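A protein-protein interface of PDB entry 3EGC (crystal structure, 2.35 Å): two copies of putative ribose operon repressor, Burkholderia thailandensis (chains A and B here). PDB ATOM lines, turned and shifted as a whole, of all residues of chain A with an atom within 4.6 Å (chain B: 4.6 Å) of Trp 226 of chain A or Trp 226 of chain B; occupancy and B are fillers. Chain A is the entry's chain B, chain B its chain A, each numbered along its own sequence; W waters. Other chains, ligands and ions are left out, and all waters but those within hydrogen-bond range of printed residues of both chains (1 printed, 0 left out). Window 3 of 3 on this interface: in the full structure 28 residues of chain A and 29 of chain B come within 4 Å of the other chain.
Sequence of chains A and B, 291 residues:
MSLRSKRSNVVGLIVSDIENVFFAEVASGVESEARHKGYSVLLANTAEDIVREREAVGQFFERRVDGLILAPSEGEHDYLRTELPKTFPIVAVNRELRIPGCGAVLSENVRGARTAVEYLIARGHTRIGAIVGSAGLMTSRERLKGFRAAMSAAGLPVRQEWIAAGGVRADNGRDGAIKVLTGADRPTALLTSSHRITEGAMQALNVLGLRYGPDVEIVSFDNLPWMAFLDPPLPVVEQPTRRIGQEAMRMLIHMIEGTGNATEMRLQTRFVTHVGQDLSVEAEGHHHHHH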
ATOM      1  N   HIS A 195      12.770 -18.255   5.110  1.00  0.00           N
ATOM      2  CA  HIS A 195      12.194 -19.462   4.531  1.00  0.00           C
ATOM      3  C   HIS A 195      10.974 -19.147   3.676  1.00  0.00           C
ATOM      4  O   HIS A 195      10.746 -19.804   2.696  1.00  0.00           O
ATOM      5  CB  HIS A 195      11.851 -20.507   5.590  1.00  0.00           C
ATOM      6  CG  HIS A 195      10.711 -20.126   6.492  1.00  0.00           C
ATOM      7  ND1 HIS A 195       9.463 -20.691   6.372  1.00  0.00           N
ATOM      8  CD2 HIS A 195      10.643 -19.271   7.551  1.00  0.00           C
ATOM      9  CE1 HIS A 195       8.685 -20.216   7.328  1.00  0.00           C
ATOM     10  NE2 HIS A 195       9.369 -19.348   8.046  1.00  0.00           N
ATOM     11  N   THR A 198      12.054 -17.884   0.496  1.00  0.00           N
ATOM     12  CA  THR A 198      12.731 -18.967  -0.205  1.00  0.00           C
ATOM     13  C   THR A 198      11.662 -19.777  -0.882  1.00  0.00           C
ATOM     14  O   THR A 198      11.851 -20.216  -2.040  1.00  0.00           O
ATOM     15  CB  THR A 198      13.596 -19.826   0.738  1.00  0.00           C
ATOM     16  OG1 THR A 198      14.679 -19.009   1.220  1.00  0.00           O
ATOM     17  CG2 THR A 198      14.163 -21.032   0.005  1.00  0.00           C
ATOM     18  N   GLU A 199      10.514 -19.930  -0.207  1.00  0.00           N
ATOM     19  CA  GLU A 199       9.367 -20.541  -0.870  1.00  0.00           C
ATOM     20  C   GLU A 199       8.974 -19.802  -2.161  1.00  0.00           C
ATOM     21  O   GLU A 199       8.660 -20.437  -3.150  1.00  0.00           O
ATOM     22  CB  GLU A 199       8.166 -20.639   0.064  1.00  0.00           C
ATOM     23  CG  GLU A 199       8.374 -21.562   1.228  1.00  0.00           C
ATOM     24  CD  GLU A 199       7.215 -21.528   2.214  1.00  0.00           C
ATOM     25  OE1 GLU A 199       6.329 -20.663   2.160  1.00  0.00           O
ATOM     26  OE2 GLU A 199       7.182 -22.394   3.059  1.00  0.00           O
ATOM     27  N   LEU A 224      15.027 -24.912   7.970  1.00  0.00           N
ATOM     28  CA  LEU A 224      13.897 -25.820   7.843  1.00  0.00           C
ATOM     29  C   LEU A 224      14.367 -27.153   7.265  1.00  0.00           C
ATOM     30  O   LEU A 224      15.102 -27.181   6.309  1.00  0.00           O
ATOM     31  CB  LEU A 224      12.853 -25.191   6.905  1.00  0.00           C
ATOM     32  CG  LEU A 224      11.881 -24.025   7.304  1.00  0.00           C
ATOM     33  CD1 LEU A 224      10.586 -24.573   7.806  1.00  0.00           C
ATOM     34  CD2 LEU A 224      12.408 -23.003   8.343  1.00  0.00           C
ATOM     35  N   PRO A 225      13.930 -28.285   7.849  1.00  0.00           N
ATOM     36  CA  PRO A 225      14.268 -29.632   7.333  1.00  0.00           C
ATOM     37  C   PRO A 225      14.035 -29.868   5.836  1.00  0.00           C
ATOM     38  O   PRO A 225      14.763 -30.618   5.212  1.00  0.00           O
ATOM     39  CB  PRO A 225      13.396 -30.573   8.187  1.00  0.00           C
ATOM     40  CG  PRO A 225      13.162 -29.817   9.463  1.00  0.00           C
ATOM     41  CD  PRO A 225      13.072 -28.356   9.038  1.00  0.00           C
ATOM     42  N   TRP A 226      13.018 -29.275   5.248  1.00  0.00           N
ATOM     43  CA  TRP A 226      12.798 -29.538   3.838  1.00  0.00           C
ATOM     44  C   TRP A 226      13.910 -29.037   2.926  1.00  0.00           C
ATOM     45  O   TRP A 226      14.160 -29.634   1.902  1.00  0.00           O
ATOM     46  CB  TRP A 226      11.414 -29.035   3.339  1.00  0.00           C
ATOM     47  CG  TRP A 226      11.254 -27.543   3.389  1.00  0.00           C
ATOM     48  CD1 TRP A 226      10.658 -26.811   4.373  1.00  0.00           C
ATOM     49  CD2 TRP A 226      11.628 -26.608   2.360  1.00  0.00           C
ATOM     50  NE1 TRP A 226      10.651 -25.479   4.034  1.00  0.00           N
ATOM     51  CE2 TRP A 226      11.242 -25.326   2.804  1.00  0.00           C
ATOM     52  CE3 TRP A 226      12.253 -26.743   1.107  1.00  0.00           C
ATOM     53  CZ2 TRP A 226      11.502 -24.157   2.063  1.00  0.00           C
ATOM     54  CZ3 TRP A 226      12.501 -25.612   0.364  1.00  0.00           C
ATOM     55  CH2 TRP A 226      12.119 -24.316   0.844  1.00  0.00           C
ATOM     56  N   MET A 227      14.536 -27.939   3.303  1.00  0.00           N
ATOM     57  CA  MET A 227      15.734 -27.411   2.606  1.00  0.00           C
ATOM     58  C   MET A 227      16.858 -28.430   2.421  1.00  0.00           C
ATOM     59  O   MET A 227      17.605 -28.329   1.456  1.00  0.00           O
ATOM     60  CB  MET A 227      16.288 -26.150   3.286  1.00  0.00           C
ATOM     61  CG  MET A 227      15.298 -25.020   3.281  1.00  0.00           C
ATOM     62  SD  MET A 227      15.764 -23.597   4.238  1.00  0.00           S
ATOM     63  CE  MET A 227      14.446 -22.449   3.938  1.00  0.00           C
ATOM     64  N   ALA A 228      16.967 -29.393   3.322  1.00  0.00           N
ATOM     65  CA  ALA A 228      17.948 -30.480   3.190  1.00  0.00           C
ATOM     66  C   ALA A 228      17.555 -31.600   2.205  1.00  0.00           C
ATOM     67  O   ALA A 228      18.312 -32.579   1.996  1.00  0.00           O
ATOM     68  CB  ALA A 228      18.252 -31.058   4.561  1.00  0.00           C
ATOM     69  N   PHE A 229      16.373 -31.509   1.598  1.00  0.00           N
ATOM     70  CA  PHE A 229      15.907 -32.628   0.826  1.00  0.00           C
ATOM     71  C   PHE A 229      16.170 -32.328  -0.584  1.00  0.00           C
ATOM     72  O   PHE A 229      16.001 -33.198  -1.407  1.00  0.00           O
ATOM     73  CB  PHE A 229      14.393 -32.863   0.900  1.00  0.00           C
ATOM     74  CG  PHE A 229      13.853 -33.119   2.289  1.00  0.00           C
ATOM     75  CD1 PHE A 229      14.631 -33.742   3.260  1.00  0.00           C
ATOM     76  CD2 PHE A 229      12.557 -32.772   2.580  1.00  0.00           C
ATOM     77  CE1 PHE A 229      14.107 -34.002   4.515  1.00  0.00           C
ATOM     78  CE2 PHE A 229      12.013 -32.997   3.823  1.00  0.00           C
ATOM     79  CZ  PHE A 229      12.787 -33.638   4.817  1.00  0.00           C
ATOM     80  N   LEU A 230      16.531 -31.091  -0.882  1.00  0.00           N
ATOM     81  CA  LEU A 230      16.722 -30.627  -2.259  1.00  0.00           C
ATOM     82  C   LEU A 230      18.066 -31.101  -2.710  1.00  0.00           C
ATOM     83  O   LEU A 230      18.884 -31.469  -1.884  1.00  0.00           O
ATOM     84  CB  LEU A 230      16.737 -29.073  -2.293  1.00  0.00           C
ATOM     85  CG  LEU A 230      15.420 -28.306  -2.503  1.00  0.00           C
ATOM     86  CD1 LEU A 230      14.183 -29.154  -2.420  1.00  0.00           C
ATOM     87  CD2 LEU A 230      15.285 -27.190  -1.518  1.00  0.00           C
ATOM     88  N   HIS B 195       2.996 -33.742   8.045  1.00  0.00           N
ATOM     89  CA  HIS B 195       4.169 -33.125   7.405  1.00  0.00           C
ATOM     90  C   HIS B 195       5.454 -33.515   8.099  1.00  0.00           C
ATOM     91  O   HIS B 195       6.464 -33.694   7.456  1.00  0.00           O
ATOM     92  CB  HIS B 195       4.039 -31.604   7.309  1.00  0.00           C
ATOM     93  CG  HIS B 195       4.092 -30.888   8.628  1.00  0.00           C
ATOM     94  ND1 HIS B 195       5.195 -30.168   9.034  1.00  0.00           N
ATOM     95  CD2 HIS B 195       3.161 -30.729   9.603  1.00  0.00           C
ATOM     96  CE1 HIS B 195       4.947 -29.606  10.213  1.00  0.00           C
ATOM     97  NE2 HIS B 195       3.720 -29.938  10.588  1.00  0.00           N
ATOM     98  N   THR B 198       6.179 -36.910   7.037  1.00  0.00           N
ATOM     99  CA  THR B 198       6.650 -36.785   5.653  1.00  0.00           C
ATOM    100  C   THR B 198       8.137 -36.380   5.590  1.00  0.00           C
ATOM    101  O   THR B 198       8.880 -36.884   4.766  1.00  0.00           O
ATOM    102  CB  THR B 198       5.795 -35.820   4.810  1.00  0.00           C
ATOM    103  OG1 THR B 198       4.435 -36.240   4.840  1.00  0.00           O
ATOM    104  CG2 THR B 198       6.291 -35.860   3.379  1.00  0.00           C
ATOM    105  N   GLU B 199       8.566 -35.488   6.495  1.00  0.00           N
ATOM    106  CA  GLU B 199      10.017 -35.187   6.609  1.00  0.00           C
ATOM    107  C   GLU B 199      10.832 -36.478   6.884  1.00  0.00           C
ATOM    108  O   GLU B 199      11.772 -36.787   6.188  1.00  0.00           O
ATOM    109  CB  GLU B 199      10.266 -34.139   7.711  1.00  0.00           C
ATOM    110  CG  GLU B 199       9.459 -32.819   7.526  1.00  0.00           C
ATOM    111  CD  GLU B 199       9.720 -31.838   8.606  1.00  0.00           C
ATOM    112  OE1 GLU B 199      10.056 -32.274   9.744  1.00  0.00           O
ATOM    113  OE2 GLU B 199       9.594 -30.619   8.320  1.00  0.00           O
ATOM    114  N   LEU B 224       1.823 -27.994   3.138  1.00  0.00           N
ATOM    115  CA  LEU B 224       2.942 -27.111   3.281  1.00  0.00           C
ATOM    116  C   LEU B 224       3.459 -26.727   1.881  1.00  0.00           C
ATOM    117  O   LEU B 224       3.608 -27.587   1.034  1.00  0.00           O
ATOM    118  CB  LEU B 224       4.029 -27.862   4.064  1.00  0.00           C
ATOM    119  CG  LEU B 224       4.015 -28.094   5.617  1.00  0.00           C
ATOM    120  CD1 LEU B 224       4.643 -26.943   6.345  1.00  0.00           C
ATOM    121  CD2 LEU B 224       2.588 -28.316   6.187  1.00  0.00           C
ATOM    122  N   PRO B 225       3.745 -25.440   1.649  1.00  0.00           N
ATOM    123  CA  PRO B 225       4.294 -24.955   0.367  1.00  0.00           C
ATOM    124  C   PRO B 225       5.458 -25.792  -0.190  1.00  0.00           C
ATOM    125  O   PRO B 225       5.445 -26.113  -1.346  1.00  0.00           O
ATOM    126  CB  PRO B 225       4.738 -23.501   0.683  1.00  0.00           C
ATOM    127  CG  PRO B 225       3.642 -23.065   1.806  1.00  0.00           C
ATOM    128  CD  PRO B 225       3.537 -24.360   2.643  1.00  0.00           C
ATOM    129  N   TRP B 226       6.417 -26.190   0.627  1.00  0.00           N
ATOM    130  CA  TRP B 226       7.517 -26.994   0.119  1.00  0.00           C
ATOM    131  C   TRP B 226       7.089 -28.276  -0.598  1.00  0.00           C
ATOM    132  O   TRP B 226       7.726 -28.686  -1.512  1.00  0.00           O
ATOM    133  CB  TRP B 226       8.590 -27.241   1.176  1.00  0.00           C
ATOM    134  CG  TRP B 226       8.196 -28.164   2.277  1.00  0.00           C
ATOM    135  CD1 TRP B 226       7.731 -27.813   3.533  1.00  0.00           C
ATOM    136  CD2 TRP B 226       8.227 -29.616   2.249  1.00  0.00           C
ATOM    137  NE1 TRP B 226       7.470 -28.941   4.253  1.00  0.00           N
ATOM    138  CE2 TRP B 226       7.769 -30.059   3.511  1.00  0.00           C
ATOM    139  CE3 TRP B 226       8.666 -30.560   1.307  1.00  0.00           C
ATOM    140  CZ2 TRP B 226       7.713 -31.394   3.859  1.00  0.00           C
ATOM    141  CZ3 TRP B 226       8.612 -31.906   1.639  1.00  0.00           C
ATOM    142  CH2 TRP B 226       8.113 -32.320   2.903  1.00  0.00           C
ATOM    143  N   MET B 227       5.961 -28.863  -0.217  1.00  0.00           N
ATOM    144  CA  MET B 227       5.477 -30.075  -0.889  1.00  0.00           C
ATOM    145  C   MET B 227       5.196 -29.871  -2.371  1.00  0.00           C
ATOM    146  O   MET B 227       5.268 -30.812  -3.179  1.00  0.00           O
ATOM    147  CB  MET B 227       4.242 -30.644  -0.207  1.00  0.00           C
ATOM    148  CG  MET B 227       4.571 -31.394   1.166  1.00  0.00           C
ATOM    149  SD  MET B 227       3.096 -31.527   2.159  1.00  0.00           S
ATOM    150  CE  MET B 227       3.989 -32.013   3.677  1.00  0.00           C
ATOM    151  N   ALA B 228       4.888 -28.635  -2.741  1.00  0.00           N
ATOM    152  CA  ALA B 228       4.675 -28.354  -4.139  1.00  0.00           C
ATOM    153  C   ALA B 228       5.976 -28.082  -4.928  1.00  0.00           C
ATOM    154  O   ALA B 228       5.921 -27.863  -6.132  1.00  0.00           O
ATOM    155  CB  ALA B 228       3.641 -27.225  -4.322  1.00  0.00           C
ATOM    156  N   PHE B 229       7.145 -28.119  -4.282  1.00  0.00           N
ATOM    157  CA  PHE B 229       8.390 -27.815  -5.041  1.00  0.00           C
ATOM    158  C   PHE B 229       8.970 -29.098  -5.541  1.00  0.00           C
ATOM    159  O   PHE B 229       9.859 -29.092  -6.352  1.00  0.00           O
ATOM    160  CB  PHE B 229       9.481 -27.126  -4.199  1.00  0.00           C
ATOM    161  CG  PHE B 229       9.027 -25.876  -3.489  1.00  0.00           C
ATOM    162  CD1 PHE B 229       8.004 -25.117  -3.989  1.00  0.00           C
ATOM    163  CD2 PHE B 229       9.641 -25.475  -2.327  1.00  0.00           C
ATOM    164  CE1 PHE B 229       7.575 -23.923  -3.290  1.00  0.00           C
ATOM    165  CE2 PHE B 229       9.235 -24.348  -1.633  1.00  0.00           C
ATOM    166  CZ  PHE B 229       8.206 -23.551  -2.107  1.00  0.00           C
ATOM    167  N   LEU B 230       8.453 -30.215  -5.033  1.00  0.00           N
ATOM    168  CA  LEU B 230       8.997 -31.530  -5.356  1.00  0.00           C
ATOM    169  C   LEU B 230       8.535 -31.980  -6.741  1.00  0.00           C
ATOM    170  O   LEU B 230       7.498 -31.537  -7.254  1.00  0.00           O
ATOM    171  CB  LEU B 230       8.552 -32.548  -4.317  1.00  0.00           C
ATOM    172  CG  LEU B 230       9.436 -32.942  -3.123  1.00  0.00           C
ATOM    173  CD1 LEU B 230      10.649 -32.026  -2.901  1.00  0.00           C
ATOM    174  CD2 LEU B 230       8.593 -33.057  -1.855  1.00  0.00           C
HETATM  175  O   HOH W   1       7.269 -25.078   3.134  1.00  0.00           O
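Glu 199 of chain A touches Pro 225 of chain B (CD to CB, 3.5 Å). Glu 199 of chain A touches Phe 229 of chain B (O to CZ, 3.3 Å). Glu 199 of chain B touches Pro 225 of chain A. CD1 of Trp 226 of chain B touches CD1 of Trp 226 of chain A (3.2 Å). CH2 of Trp 226 of chain A touches CE2 of Phe 229 of chain B (3.8 Å). Phe 229 of chain A touches Glu 199 of chain B (CZ to O, 3.6 Å).
Of chain B, only Trp 226 and Phe 229 come within 4 Å of Trp 226 of chain A. Trp 226 of chain B touches one residue of chain A. Printed residues of chain A within 4 Å of Pro 225 of chain B: Glu 199. Printed residues of chain A within 4 Å of Glu 199 of chain B: Pro 225 and Phe 229. Printed residues of chain B within 4 Å of Glu 199 of chain A: Pro 225 and Phe 229. Printed residues of chain B within 4 Å of Phe 229 of chain A: Glu 199. Ala 228 of chain B touches none of the printed residues of chain A. Met 227 of chain B touches none of the printed residues of chain A. The nearest residue of chain A that does not touch Trp 226 of chain B is Phe 229 of chain A (4.1 Å). The nearest printed residue of chain A that does not touch Pro 225 of chain B is Trp 226 of chain A (6.5 Å).
Of the 10 printed residues of chain A, 4 touch a printed residue of chain B. Among the printed residues, 6 pairs touch across the chains. Among the printed residues, no Asp or Glu carboxylate lies within 4 Å of a Lys or Arg side-chain nitrogen of the other chain.
Glu 199 of chain A touches Pro 225 of chain B, and with the chains exchanged Pro 225 of chain A touches Glu 199 of chain B. Glu 199 of chain A touches Phe 229 of chain B, and with the chains exchanged Phe 229 of chain A touches Glu 199 of chain B. Trp 226 of chain A touches its own counterpart, Trp 226 of chain B. Trp 226 of chain A touches Phe 229 of chain B, but with the chains exchanged Phe 229 of chain A does not touch Trp 226 of chain B (4.1 Å). Positions printed for both chains: 195, 198, 199, 224, 225, 226, 227, 228, 229 and 230.
Water W1 bridges OE2 of Glu 199 of chain A and N of Trp 226 of chain B.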
